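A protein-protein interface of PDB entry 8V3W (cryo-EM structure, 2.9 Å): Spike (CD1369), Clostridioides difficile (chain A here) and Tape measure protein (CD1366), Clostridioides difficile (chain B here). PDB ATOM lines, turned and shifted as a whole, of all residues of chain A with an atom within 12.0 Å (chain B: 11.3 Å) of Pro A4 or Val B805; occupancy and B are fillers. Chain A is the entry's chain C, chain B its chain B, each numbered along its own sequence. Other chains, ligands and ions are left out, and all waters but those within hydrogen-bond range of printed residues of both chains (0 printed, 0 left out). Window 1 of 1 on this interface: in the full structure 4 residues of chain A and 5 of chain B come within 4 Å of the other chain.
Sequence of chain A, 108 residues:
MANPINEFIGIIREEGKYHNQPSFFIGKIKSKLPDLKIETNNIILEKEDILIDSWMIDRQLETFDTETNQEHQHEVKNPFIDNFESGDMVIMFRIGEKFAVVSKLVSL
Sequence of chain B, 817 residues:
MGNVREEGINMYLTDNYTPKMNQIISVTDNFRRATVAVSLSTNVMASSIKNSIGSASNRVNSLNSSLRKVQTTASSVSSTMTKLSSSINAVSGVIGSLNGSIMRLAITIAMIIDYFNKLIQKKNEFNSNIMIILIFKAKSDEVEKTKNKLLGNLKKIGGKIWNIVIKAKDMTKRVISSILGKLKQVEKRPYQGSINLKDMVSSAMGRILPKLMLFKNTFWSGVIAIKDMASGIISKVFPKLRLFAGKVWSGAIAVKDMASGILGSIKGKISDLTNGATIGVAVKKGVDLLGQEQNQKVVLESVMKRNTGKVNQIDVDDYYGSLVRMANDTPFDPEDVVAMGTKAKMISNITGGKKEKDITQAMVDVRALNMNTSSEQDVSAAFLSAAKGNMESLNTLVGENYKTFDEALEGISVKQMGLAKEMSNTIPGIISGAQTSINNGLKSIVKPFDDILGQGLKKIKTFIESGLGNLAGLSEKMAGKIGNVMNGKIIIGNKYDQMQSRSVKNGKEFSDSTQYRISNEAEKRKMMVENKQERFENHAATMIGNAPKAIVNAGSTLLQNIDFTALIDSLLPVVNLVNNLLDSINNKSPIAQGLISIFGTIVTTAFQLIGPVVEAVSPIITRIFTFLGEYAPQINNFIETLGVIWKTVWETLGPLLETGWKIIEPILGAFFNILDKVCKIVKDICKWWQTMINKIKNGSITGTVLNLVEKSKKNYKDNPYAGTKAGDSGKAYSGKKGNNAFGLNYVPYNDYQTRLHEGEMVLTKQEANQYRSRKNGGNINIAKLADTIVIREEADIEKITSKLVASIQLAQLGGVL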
ATOM      1  N   ALA A   2       9.472 -14.591  23.433  1.00  0.00           N
ATOM      2  CA  ALA A   2       9.612 -16.024  23.640  1.00  0.00           C
ATOM      3  C   ALA A   2      11.077 -16.430  23.756  1.00  0.00           C
ATOM      4  O   ALA A   2      11.839 -16.314  22.802  1.00  0.00           O
ATOM      5  CB  ALA A   2       8.947 -16.784  22.514  1.00  0.00           C
ATOM      6  N   ASN A   3      11.457 -16.904  24.931  1.00  0.00           N
ATOM      7  CA  ASN A   3      12.799 -17.422  25.152  1.00  0.00           C
ATOM      8  C   ASN A   3      12.946 -18.779  24.471  1.00  0.00           C
ATOM      9  O   ASN A   3      12.122 -19.668  24.697  1.00  0.00           O
ATOM     10  CB  ASN A   3      13.072 -17.545  26.646  1.00  0.00           C
ATOM     11  CG  ASN A   3      14.484 -17.975  26.949  1.00  0.00           C
ATOM     12  OD1 ASN A   3      14.748 -19.150  27.176  1.00  0.00           O
ATOM     13  ND2 ASN A   3      15.400 -17.022  26.971  1.00  0.00           N
ATOM     14  N   PRO A   4      13.963 -18.968  23.625  1.00  0.00           N
ATOM     15  CA  PRO A   4      14.082 -20.237  22.884  1.00  0.00           C
ATOM     16  C   PRO A   4      14.251 -21.475  23.754  1.00  0.00           C
ATOM     17  O   PRO A   4      13.807 -22.555  23.350  1.00  0.00           O
ATOM     18  CB  PRO A   4      15.311 -20.007  21.992  1.00  0.00           C
ATOM     19  CG  PRO A   4      16.005 -18.819  22.562  1.00  0.00           C
ATOM     20  CD  PRO A   4      14.955 -17.977  23.188  1.00  0.00           C
ATOM     21  N   ILE A   5      14.886 -21.366  24.923  1.00  0.00           N
ATOM     22  CA  ILE A   5      15.064 -22.537  25.780  1.00  0.00           C
ATOM     23  C   ILE A   5      13.718 -23.058  26.276  1.00  0.00           C
ATOM     24  O   ILE A   5      13.467 -24.271  26.276  1.00  0.00           O
ATOM     25  CB  ILE A   5      16.004 -22.204  26.952  1.00  0.00           C
ATOM     26  CG1 ILE A   5      17.400 -21.847  26.444  1.00  0.00           C
ATOM     27  CG2 ILE A   5      16.087 -23.368  27.912  1.00  0.00           C
ATOM     28  CD1 ILE A   5      18.158 -23.011  25.868  1.00  0.00           C
ATOM     29  N   ASN A   6      12.836 -22.156  26.709  1.00  0.00           N
ATOM     30  CA  ASN A   6      11.513 -22.568  27.165  1.00  0.00           C
ATOM     31  C   ASN A   6      10.710 -23.197  26.036  1.00  0.00           C
ATOM     32  O   ASN A   6       9.974 -24.167  26.249  1.00  0.00           O
ATOM     33  CB  ASN A   6      10.765 -21.372  27.751  1.00  0.00           C
ATOM     34  CG  ASN A   6      11.508 -20.722  28.897  1.00  0.00           C
ATOM     35  OD1 ASN A   6      12.605 -21.140  29.259  1.00  0.00           O
ATOM     36  ND2 ASN A   6      10.913 -19.690  29.475  1.00  0.00           N
ATOM     37  N   GLU A   7      10.828 -22.648  24.826  1.00  0.00           N
ATOM     38  CA  GLU A   7      10.139 -23.226  23.681  1.00  0.00           C
ATOM     39  C   GLU A   7      10.662 -24.619  23.373  1.00  0.00           C
ATOM     40  O   GLU A   7       9.887 -25.519  23.034  1.00  0.00           O
ATOM     41  CB  GLU A   7      10.292 -22.316  22.467  1.00  0.00           C
ATOM     42  CG  GLU A   7       9.737 -20.925  22.668  1.00  0.00           C
ATOM     43  CD  GLU A   7       8.225 -20.906  22.678  1.00  0.00           C
ATOM     44  OE1 GLU A   7       7.622 -21.519  21.775  1.00  0.00           O
ATOM     45  OE2 GLU A   7       7.638 -20.279  23.583  1.00  0.00           O
ATOM     46  N   PHE A   8      11.976 -24.817  23.482  1.00  0.00           N
ATOM     47  CA  PHE A   8      12.552 -26.140  23.269  1.00  0.00           C
ATOM     48  C   PHE A   8      12.043 -27.138  24.302  1.00  0.00           C
ATOM     49  O   PHE A   8      11.721 -28.284  23.964  1.00  0.00           O
ATOM     50  CB  PHE A   8      14.075 -26.049  23.312  1.00  0.00           C
ATOM     51  CG  PHE A   8      14.769 -27.278  22.815  1.00  0.00           C
ATOM     52  CD1 PHE A   8      14.626 -27.683  21.502  1.00  0.00           C
ATOM     53  CD2 PHE A   8      15.571 -28.023  23.656  1.00  0.00           C
ATOM     54  CE1 PHE A   8      15.260 -28.808  21.042  1.00  0.00           C
ATOM     55  CE2 PHE A   8      16.208 -29.149  23.198  1.00  0.00           C
ATOM     56  CZ  PHE A   8      16.053 -29.541  21.890  1.00  0.00           C
ATOM     57  N   ILE A   9      11.966 -26.721  25.567  1.00  0.00           N
ATOM     58  CA  ILE A   9      11.463 -27.611  26.612  1.00  0.00           C
ATOM     59  C   ILE A   9      10.005 -27.970  26.349  1.00  0.00           C
ATOM     60  O   ILE A   9       9.597 -29.129  26.497  1.00  0.00           O
ATOM     61  CB  ILE A   9      11.657 -26.973  28.000  1.00  0.00           C
ATOM     62  CG1 ILE A   9      13.138 -26.959  28.374  1.00  0.00           C
ATOM     63  CG2 ILE A   9      10.885 -27.736  29.050  1.00  0.00           C
ATOM     64  CD1 ILE A   9      13.474 -26.062  29.532  1.00  0.00           C
ATOM     65  N   GLY A  10       9.198 -26.985  25.948  1.00  0.00           N
ATOM     66  CA  GLY A  10       7.812 -27.273  25.605  1.00  0.00           C
ATOM     67  C   GLY A  10       7.680 -28.216  24.424  1.00  0.00           C
ATOM     68  O   GLY A  10       6.805 -29.084  24.403  1.00  0.00           O
ATOM     69  N   ILE A  11       8.551 -28.059  23.426  1.00  0.00           N
ATOM     70  CA  ILE A  11       8.554 -28.954  22.273  1.00  0.00           C
ATOM     71  C   ILE A  11       8.873 -30.379  22.703  1.00  0.00           C
ATOM     72  O   ILE A  11       8.244 -31.337  22.241  1.00  0.00           O
ATOM     73  CB  ILE A  11       9.546 -28.443  21.214  1.00  0.00           C
ATOM     74  CG1 ILE A  11       8.926 -27.304  20.406  1.00  0.00           C
ATOM     75  CG2 ILE A  11      10.001 -29.570  20.307  1.00  0.00           C
ATOM     76  CD1 ILE A  11       9.850 -26.728  19.374  1.00  0.00           C
ATOM     77  N   ILE A  12       9.863 -30.544  23.583  1.00  0.00           N
ATOM     78  CA  ILE A  12      10.198 -31.879  24.077  1.00  0.00           C
ATOM     79  C   ILE A  12       9.012 -32.486  24.812  1.00  0.00           C
ATOM     80  O   ILE A  12       8.648 -33.648  24.592  1.00  0.00           O
ATOM     81  CB  ILE A  12      11.442 -31.825  24.981  1.00  0.00           C
ATOM     82  CG1 ILE A  12      12.673 -31.403  24.185  1.00  0.00           C
ATOM     83  CG2 ILE A  12      11.673 -33.166  25.636  1.00  0.00           C
ATOM     84  CD1 ILE A  12      13.907 -31.259  25.028  1.00  0.00           C
ATOM     85  N   ARG A  13       8.386 -31.703  25.693  1.00  0.00           N
ATOM     86  CA  ARG A  13       7.258 -32.218  26.462  1.00  0.00           C
ATOM     87  C   ARG A  13       6.110 -32.633  25.549  1.00  0.00           C
ATOM     88  O   ARG A  13       5.442 -33.639  25.805  1.00  0.00           O
ATOM     89  CB  ARG A  13       6.785 -31.178  27.474  1.00  0.00           C
ATOM     90  CG  ARG A  13       7.752 -30.927  28.613  1.00  0.00           C
ATOM     91  CD  ARG A  13       7.378 -29.667  29.364  1.00  0.00           C
ATOM     92  NE  ARG A  13       8.077 -29.554  30.637  1.00  0.00           N
ATOM     93  CZ  ARG A  13       7.855 -28.599  31.528  1.00  0.00           C
ATOM     94  NH1 ARG A  13       6.954 -27.655  31.317  1.00  0.00           N
ATOM     95  NH2 ARG A  13       8.555 -28.588  32.657  1.00  0.00           N
ATOM     96  N   GLU A  14       5.859 -31.867  24.486  1.00  0.00           N
ATOM     97  CA  GLU A  14       4.760 -32.212  23.589  1.00  0.00           C
ATOM     98  C   GLU A  14       5.090 -33.421  22.722  1.00  0.00           C
ATOM     99  O   GLU A  14       4.252 -34.313  22.557  1.00  0.00           O
ATOM    100  CB  GLU A  14       4.391 -31.014  22.717  1.00  0.00           C
ATOM    101  CG  GLU A  14       3.770 -29.868  23.489  1.00  0.00           C
ATOM    102  CD  GLU A  14       2.360 -30.162  23.961  1.00  0.00           C
ATOM    103  OE1 GLU A  14       1.806 -31.216  23.584  1.00  0.00           O
ATOM    104  OE2 GLU A  14       1.804 -29.337  24.716  1.00  0.00           O
ATOM    105  N   GLU A  15       6.294 -33.472  22.149  1.00  0.00           N
ATOM    106  CA  GLU A  15       6.645 -34.576  21.263  1.00  0.00           C
ATOM    107  C   GLU A  15       6.886 -35.877  22.011  1.00  0.00           C
ATOM    108  O   GLU A  15       6.878 -36.941  21.386  1.00  0.00           O
ATOM    109  CB  GLU A  15       7.886 -34.236  20.436  1.00  0.00           C
ATOM    110  CG  GLU A  15       7.655 -33.212  19.343  1.00  0.00           C
ATOM    111  CD  GLU A  15       6.747 -33.724  18.245  1.00  0.00           C
ATOM    112  OE1 GLU A  15       6.686 -34.953  18.047  1.00  0.00           O
ATOM    113  OE2 GLU A  15       6.100 -32.897  17.571  1.00  0.00           O
ATOM    114  N   ALA B 795      26.199 -15.724  23.343  1.00  0.00           N
ATOM    115  CA  ALA B 795      24.926 -15.484  22.674  1.00  0.00           C
ATOM    116  C   ALA B 795      24.768 -16.385  21.455  1.00  0.00           C
ATOM    117  O   ALA B 795      23.682 -16.491  20.892  1.00  0.00           O
ATOM    118  CB  ALA B 795      24.807 -14.027  22.271  1.00  0.00           C
ATOM    119  N   ASP B 796      25.865 -17.027  21.052  1.00  0.00           N
ATOM    120  CA  ASP B 796      25.816 -17.929  19.906  1.00  0.00           C
ATOM    121  C   ASP B 796      24.849 -19.076  20.158  1.00  0.00           C
ATOM    122  O   ASP B 796      24.109 -19.491  19.256  1.00  0.00           O
ATOM    123  CB  ASP B 796      27.216 -18.463  19.609  1.00  0.00           C
ATOM    124  CG  ASP B 796      27.448 -18.704  18.135  1.00  0.00           C
ATOM    125  OD1 ASP B 796      26.779 -18.046  17.312  1.00  0.00           O
ATOM    126  OD2 ASP B 796      28.301 -19.554  17.800  1.00  0.00           O
ATOM    127  N   ILE B 797      24.837 -19.594  21.387  1.00  0.00           N
ATOM    128  CA  ILE B 797      23.946 -20.696  21.727  1.00  0.00           C
ATOM    129  C   ILE B 797      22.492 -20.270  21.586  1.00  0.00           C
ATOM    130  O   ILE B 797      21.643 -21.053  21.145  1.00  0.00           O
ATOM    131  CB  ILE B 797      24.262 -21.215  23.144  1.00  0.00           C
ATOM    132  CG1 ILE B 797      23.279 -22.310  23.548  1.00  0.00           C
ATOM    133  CG2 ILE B 797      24.256 -20.076  24.149  1.00  0.00           C
ATOM    134  CD1 ILE B 797      23.367 -23.543  22.676  1.00  0.00           C
ATOM    135  N   GLU B 798      22.178 -19.022  21.941  1.00  0.00           N
ATOM    136  CA  GLU B 798      20.804 -18.543  21.811  1.00  0.00           C
ATOM    137  C   GLU B 798      20.368 -18.479  20.353  1.00  0.00           C
ATOM    138  O   GLU B 798      19.246 -18.878  20.020  1.00  0.00           O
ATOM    139  CB  GLU B 798      20.657 -17.178  22.477  1.00  0.00           C
ATOM    140  CG  GLU B 798      20.654 -17.231  23.992  1.00  0.00           C
ATOM    141  CD  GLU B 798      19.263 -17.069  24.577  1.00  0.00           C
ATOM    142  OE1 GLU B 798      18.577 -16.090  24.216  1.00  0.00           O
ATOM    143  OE2 GLU B 798      18.856 -17.916  25.400  1.00  0.00           O
ATOM    144  N   LYS B 799      21.232 -17.978  19.468  1.00  0.00           N
ATOM    145  CA  LYS B 799      20.884 -17.922  18.051  1.00  0.00           C
ATOM    146  C   LYS B 799      20.725 -19.318  17.463  1.00  0.00           C
ATOM    147  O   LYS B 799      19.797 -19.572  16.680  1.00  0.00           O
ATOM    148  CB  LYS B 799      21.941 -17.134  17.285  1.00  0.00           C
ATOM    149  CG  LYS B 799      22.252 -15.789  17.898  1.00  0.00           C
ATOM    150  CD  LYS B 799      21.343 -14.712  17.337  1.00  0.00           C
ATOM    151  CE  LYS B 799      21.005 -13.681  18.394  1.00  0.00           C
ATOM    152  NZ  LYS B 799      22.220 -12.965  18.865  1.00  0.00           N
ATOM    153  N   ILE B 800      21.618 -20.237  17.836  1.00  0.00           N
ATOM    154  CA  ILE B 800      21.513 -21.609  17.350  1.00  0.00           C
ATOM    155  C   ILE B 800      20.215 -22.245  17.831  1.00  0.00           C
ATOM    156  O   ILE B 800      19.525 -22.936  17.070  1.00  0.00           O
ATOM    157  CB  ILE B 800      22.749 -22.416  17.783  1.00  0.00           C
ATOM    158  CG1 ILE B 800      23.990 -21.888  17.067  1.00  0.00           C
ATOM    159  CG2 ILE B 800      22.564 -23.890  17.488  1.00  0.00           C
ATOM    160  CD1 ILE B 800      25.270 -22.560  17.486  1.00  0.00           C
ATOM    161  N   THR B 801      19.857 -22.018  19.097  1.00  0.00           N
ATOM    162  CA  THR B 801      18.619 -22.573  19.629  1.00  0.00           C
ATOM    163  C   THR B 801      17.404 -21.985  18.926  1.00  0.00           C
ATOM    164  O   THR B 801      16.431 -22.696  18.659  1.00  0.00           O
ATOM    165  CB  THR B 801      18.538 -22.326  21.134  1.00  0.00           C
ATOM    166  OG1 THR B 801      19.838 -22.471  21.714  1.00  0.00           O
ATOM    167  CG2 THR B 801      17.594 -23.316  21.784  1.00  0.00           C
ATOM    168  N   SER B 802      17.441 -20.687  18.622  1.00  0.00           N
ATOM    169  CA  SER B 802      16.330 -20.064  17.910  1.00  0.00           C
ATOM    170  C   SER B 802      16.145 -20.687  16.533  1.00  0.00           C
ATOM    171  O   SER B 802      15.017 -20.997  16.122  1.00  0.00           O
ATOM    172  CB  SER B 802      16.569 -18.560  17.791  1.00  0.00           C
ATOM    173  OG  SER B 802      16.225 -17.900  18.993  1.00  0.00           O
ATOM    174  N   LYS B 803      17.245 -20.882  15.806  1.00  0.00           N
ATOM    175  CA  LYS B 803      17.148 -21.493  14.483  1.00  0.00           C
ATOM    176  C   LYS B 803      16.633 -22.926  14.569  1.00  0.00           C
ATOM    177  O   LYS B 803      15.785 -23.341  13.765  1.00  0.00           O
ATOM    178  CB  LYS B 803      18.504 -21.445  13.787  1.00  0.00           C
ATOM    179  CG  LYS B 803      18.926 -20.047  13.391  1.00  0.00           C
ATOM    180  CD  LYS B 803      20.388 -19.992  13.011  1.00  0.00           C
ATOM    181  CE  LYS B 803      20.816 -18.573  12.681  1.00  0.00           C
ATOM    182  NZ  LYS B 803      22.282 -18.468  12.449  1.00  0.00           N
ATOM    183  N   LEU B 804      17.124 -23.693  15.542  1.00  0.00           N
ATOM    184  CA  LEU B 804      16.663 -25.067  15.704  1.00  0.00           C
ATOM    185  C   LEU B 804      15.174 -25.119  16.024  1.00  0.00           C
ATOM    186  O   LEU B 804      14.442 -25.949  15.470  1.00  0.00           O
ATOM    187  CB  LEU B 804      17.483 -25.755  16.794  1.00  0.00           C
ATOM    188  CG  LEU B 804      17.219 -27.229  17.084  1.00  0.00           C
ATOM    189  CD1 LEU B 804      17.453 -28.068  15.845  1.00  0.00           C
ATOM    190  CD2 LEU B 804      18.108 -27.694  18.216  1.00  0.00           C
ATOM    191  N   VAL B 805      14.703 -24.230  16.900  1.00  0.00           N
ATOM    192  CA  VAL B 805      13.288 -24.204  17.258  1.00  0.00           C
ATOM    193  C   VAL B 805      12.429 -23.861  16.046  1.00  0.00           C
ATOM    194  O   VAL B 805      11.388 -24.488  15.809  1.00  0.00           O
ATOM    195  CB  VAL B 805      13.053 -23.224  18.421  1.00  0.00           C
ATOM    196  CG1 VAL B 805      11.580 -22.896  18.559  1.00  0.00           C
ATOM    197  CG2 VAL B 805      13.579 -23.810  19.712  1.00  0.00           C
ATOM    198  N   ALA B 806      12.847 -22.865  15.259  1.00  0.00           N
ATOM    199  CA  ALA B 806      12.076 -22.506  14.071  1.00  0.00           C
ATOM    200  C   ALA B 806      11.999 -23.667  13.085  1.00  0.00           C
ATOM    201  O   ALA B 806      10.926 -23.957  12.530  1.00  0.00           O
ATOM    202  CB  ALA B 806      12.682 -21.276  13.403  1.00  0.00           C
ATOM    203  N   SER B 807      13.123 -24.350  12.862  1.00  0.00           N
ATOM    204  CA  SER B 807      13.126 -25.485  11.944  1.00  0.00           C
ATOM    205  C   SER B 807      12.212 -26.600  12.436  1.00  0.00           C
ATOM    206  O   SER B 807      11.455 -27.187  11.649  1.00  0.00           O
ATOM    207  CB  SER B 807      14.551 -26.000  11.763  1.00  0.00           C
ATOM    208  OG  SER B 807      15.397 -24.972  11.286  1.00  0.00           O
ATOM    209  N   ILE B 808      12.257 -26.898  13.735  1.00  0.00           N
ATOM    210  CA  ILE B 808      11.422 -27.964  14.278  1.00  0.00           C
ATOM    211  C   ILE B 808       9.947 -27.612  14.143  1.00  0.00           C
ATOM    212  O   ILE B 808       9.121 -28.473  13.825  1.00  0.00           O
ATOM    213  CB  ILE B 808      11.804 -28.254  15.740  1.00  0.00           C
ATOM    214  CG1 ILE B 808      13.204 -28.854  15.814  1.00  0.00           C
ATOM    215  CG2 ILE B 808      10.807 -29.197  16.374  1.00  0.00           C
ATOM    216  CD1 ILE B 808      13.633 -29.216  17.206  1.00  0.00           C
ATOM    217  N   GLN B 809       9.587 -26.350  14.389  1.00  0.00           N
ATOM    218  CA  GLN B 809       8.185 -25.956  14.270  1.00  0.00           C
ATOM    219  C   GLN B 809       7.692 -26.067  12.831  1.00  0.00           C
ATOM    220  O   GLN B 809       6.574 -26.540  12.581  1.00  0.00           O
ATOM    221  CB  GLN B 809       7.990 -24.539  14.801  1.00  0.00           C
ATOM    222  CG  GLN B 809       7.875 -24.473  16.307  1.00  0.00           C
ATOM    223  CD  GLN B 809       8.191 -23.102  16.850  1.00  0.00           C
ATOM    224  OE1 GLN B 809       8.894 -22.321  16.214  1.00  0.00           O
ATOM    225  NE2 GLN B 809       7.691 -22.807  18.042  1.00  0.00           N
ATOM    226  N   LEU B 810       8.513 -25.638  11.868  1.00  0.00           N
ATOM    227  CA  LEU B 810       8.127 -25.796  10.468  1.00  0.00           C
ATOM    228  C   LEU B 810       7.930 -27.265  10.114  1.00  0.00           C
ATOM    229  O   LEU B 810       6.950 -27.626   9.449  1.00  0.00           O
ATOM    230  CB  LEU B 810       9.176 -25.164   9.557  1.00  0.00           C
ATOM    231  CG  LEU B 810       8.828 -25.127   8.069  1.00  0.00           C
ATOM    232  CD1 LEU B 810       7.575 -24.311   7.821  1.00  0.00           C
ATOM    233  CD2 LEU B 810       9.993 -24.595   7.252  1.00  0.00           C
ATOM    234  N   ALA B 811       8.842 -28.129  10.566  1.00  0.00           N
ATOM    235  CA  ALA B 811       8.718 -29.552  10.272  1.00  0.00           C
ATOM    236  C   ALA B 811       7.475 -30.150  10.920  1.00  0.00           C
ATOM    237  O   ALA B 811       6.825 -31.023  10.337  1.00  0.00           O
ATOM    238  CB  ALA B 811       9.972 -30.294  10.728  1.00  0.00           C
ATOM    239  N   GLN B 812       7.135 -29.702  12.130  1.00  0.00           N
ATOM    240  CA  GLN B 812       5.916 -30.178  12.775  1.00  0.00           C
ATOM    241  C   GLN B 812       4.684 -29.790  11.974  1.00  0.00           C
ATOM    242  O   GLN B 812       3.752 -30.586  11.834  1.00  0.00           O
ATOM    243  CB  GLN B 812       5.807 -29.621  14.192  1.00  0.00           C
ATOM    244  CG  GLN B 812       6.688 -30.282  15.219  1.00  0.00           C
ATOM    245  CD  GLN B 812       6.509 -29.663  16.584  1.00  0.00           C
ATOM    246  OE1 GLN B 812       6.270 -28.463  16.705  1.00  0.00           O
ATOM    247  NE2 GLN B 812       6.614 -30.477  17.622  1.00  0.00           N
ATOM    248  N   LEU B 813       4.650 -28.555  11.465  1.00  0.00           N
ATOM    249  CA  LEU B 813       3.520 -28.147  10.635  1.00  0.00           C
ATOM    250  C   LEU B 813       3.437 -28.996   9.374  1.00  0.00           C
ATOM    251  O   LEU B 813       2.348 -29.418   8.970  1.00  0.00           O
ATOM    252  CB  LEU B 813       3.629 -26.661  10.283  1.00  0.00           C
ATOM    253  CG  LEU B 813       2.524 -25.958   9.478  1.00  0.00           C
ATOM    254  CD1 LEU B 813       2.753 -26.069   7.983  1.00  0.00           C
ATOM    255  CD2 LEU B 813       1.134 -26.458   9.839  1.00  0.00           C
ATOM    256  N   GLY B 814       4.580 -29.269   8.742  1.00  0.00           N
ATOM    257  CA  GLY B 814       4.574 -30.044   7.514  1.00  0.00           C
ATOM    258  C   GLY B 814       4.188 -31.499   7.688  1.00  0.00           C
ATOM    259  O   GLY B 814       3.776 -32.138   6.716  1.00  0.00           O
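OE2 of Glu A15 lies within hydrogen-bond range of NE2 of Gln B812, 2.5 Å away.
Of chain B, only Ser B802 and Val B805 come within 4 Å of Pro A4. Val B805 touches just one residue of chain A: Pro A4 (3.9 Å). No residue of chain B comes within 4 Å of Asn A6. Glu B798 touches just one residue of chain A: Asn A3 (3.9 Å). No residue of chain A comes within 4 Å of Thr B801. Ser B802 touches one residue of chain A. No residue of chain A comes within 4 Å of Leu B804. No residue of chain A comes within 4 Å of Ala B806. Gln B809 touches one residue of chain A. Printed residues of chain B within 4 Å of Glu A15: Gln B812 (2.5 Å). Of the printed residues of chain A, Gln B812 touches Glu A15. Arg A13 touches none of the printed residues of chain B. The nearest residue of chain B that does not touch Pro A4 is Thr B801 (4.03 Å). The nearest residue of chain A that does not touch Val B805 is Glu A7 (4.2 Å).
Among the printed residues, merely in contact across the chains: Asn A3 with Glu B798, Pro A4 with Ser B802, Pro A4 with Val B805 and Glu A7 with Gln B809.
Of the 20 printed residues of chain B, 5 touch a printed residue of chain A. Hydrophobic or aromatic side chains of chain B within 4 Å of the printed part of chain A: Val B805. Hydrophobic or aromatic side chains of chain A that line the printed part of chain B: Pro A4. Among the printed residues, 5 pairs touch across the chains.
The side-chain amide oxygen (OD1) of Asn A3 sits at hydrogen-bond distance from the backbone NH (N) of Ile A5 (3.2 Å). The backbone carbonyl oxygen of Glu B798 sits at hydrogen-bond distance from the side-chain hydroxyl of Ser B802 (3.3 Å). The backbone carbonyl oxygen (O) of Val B805 lies close to the side-chain amide oxygen (OE1) of Gln B809.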
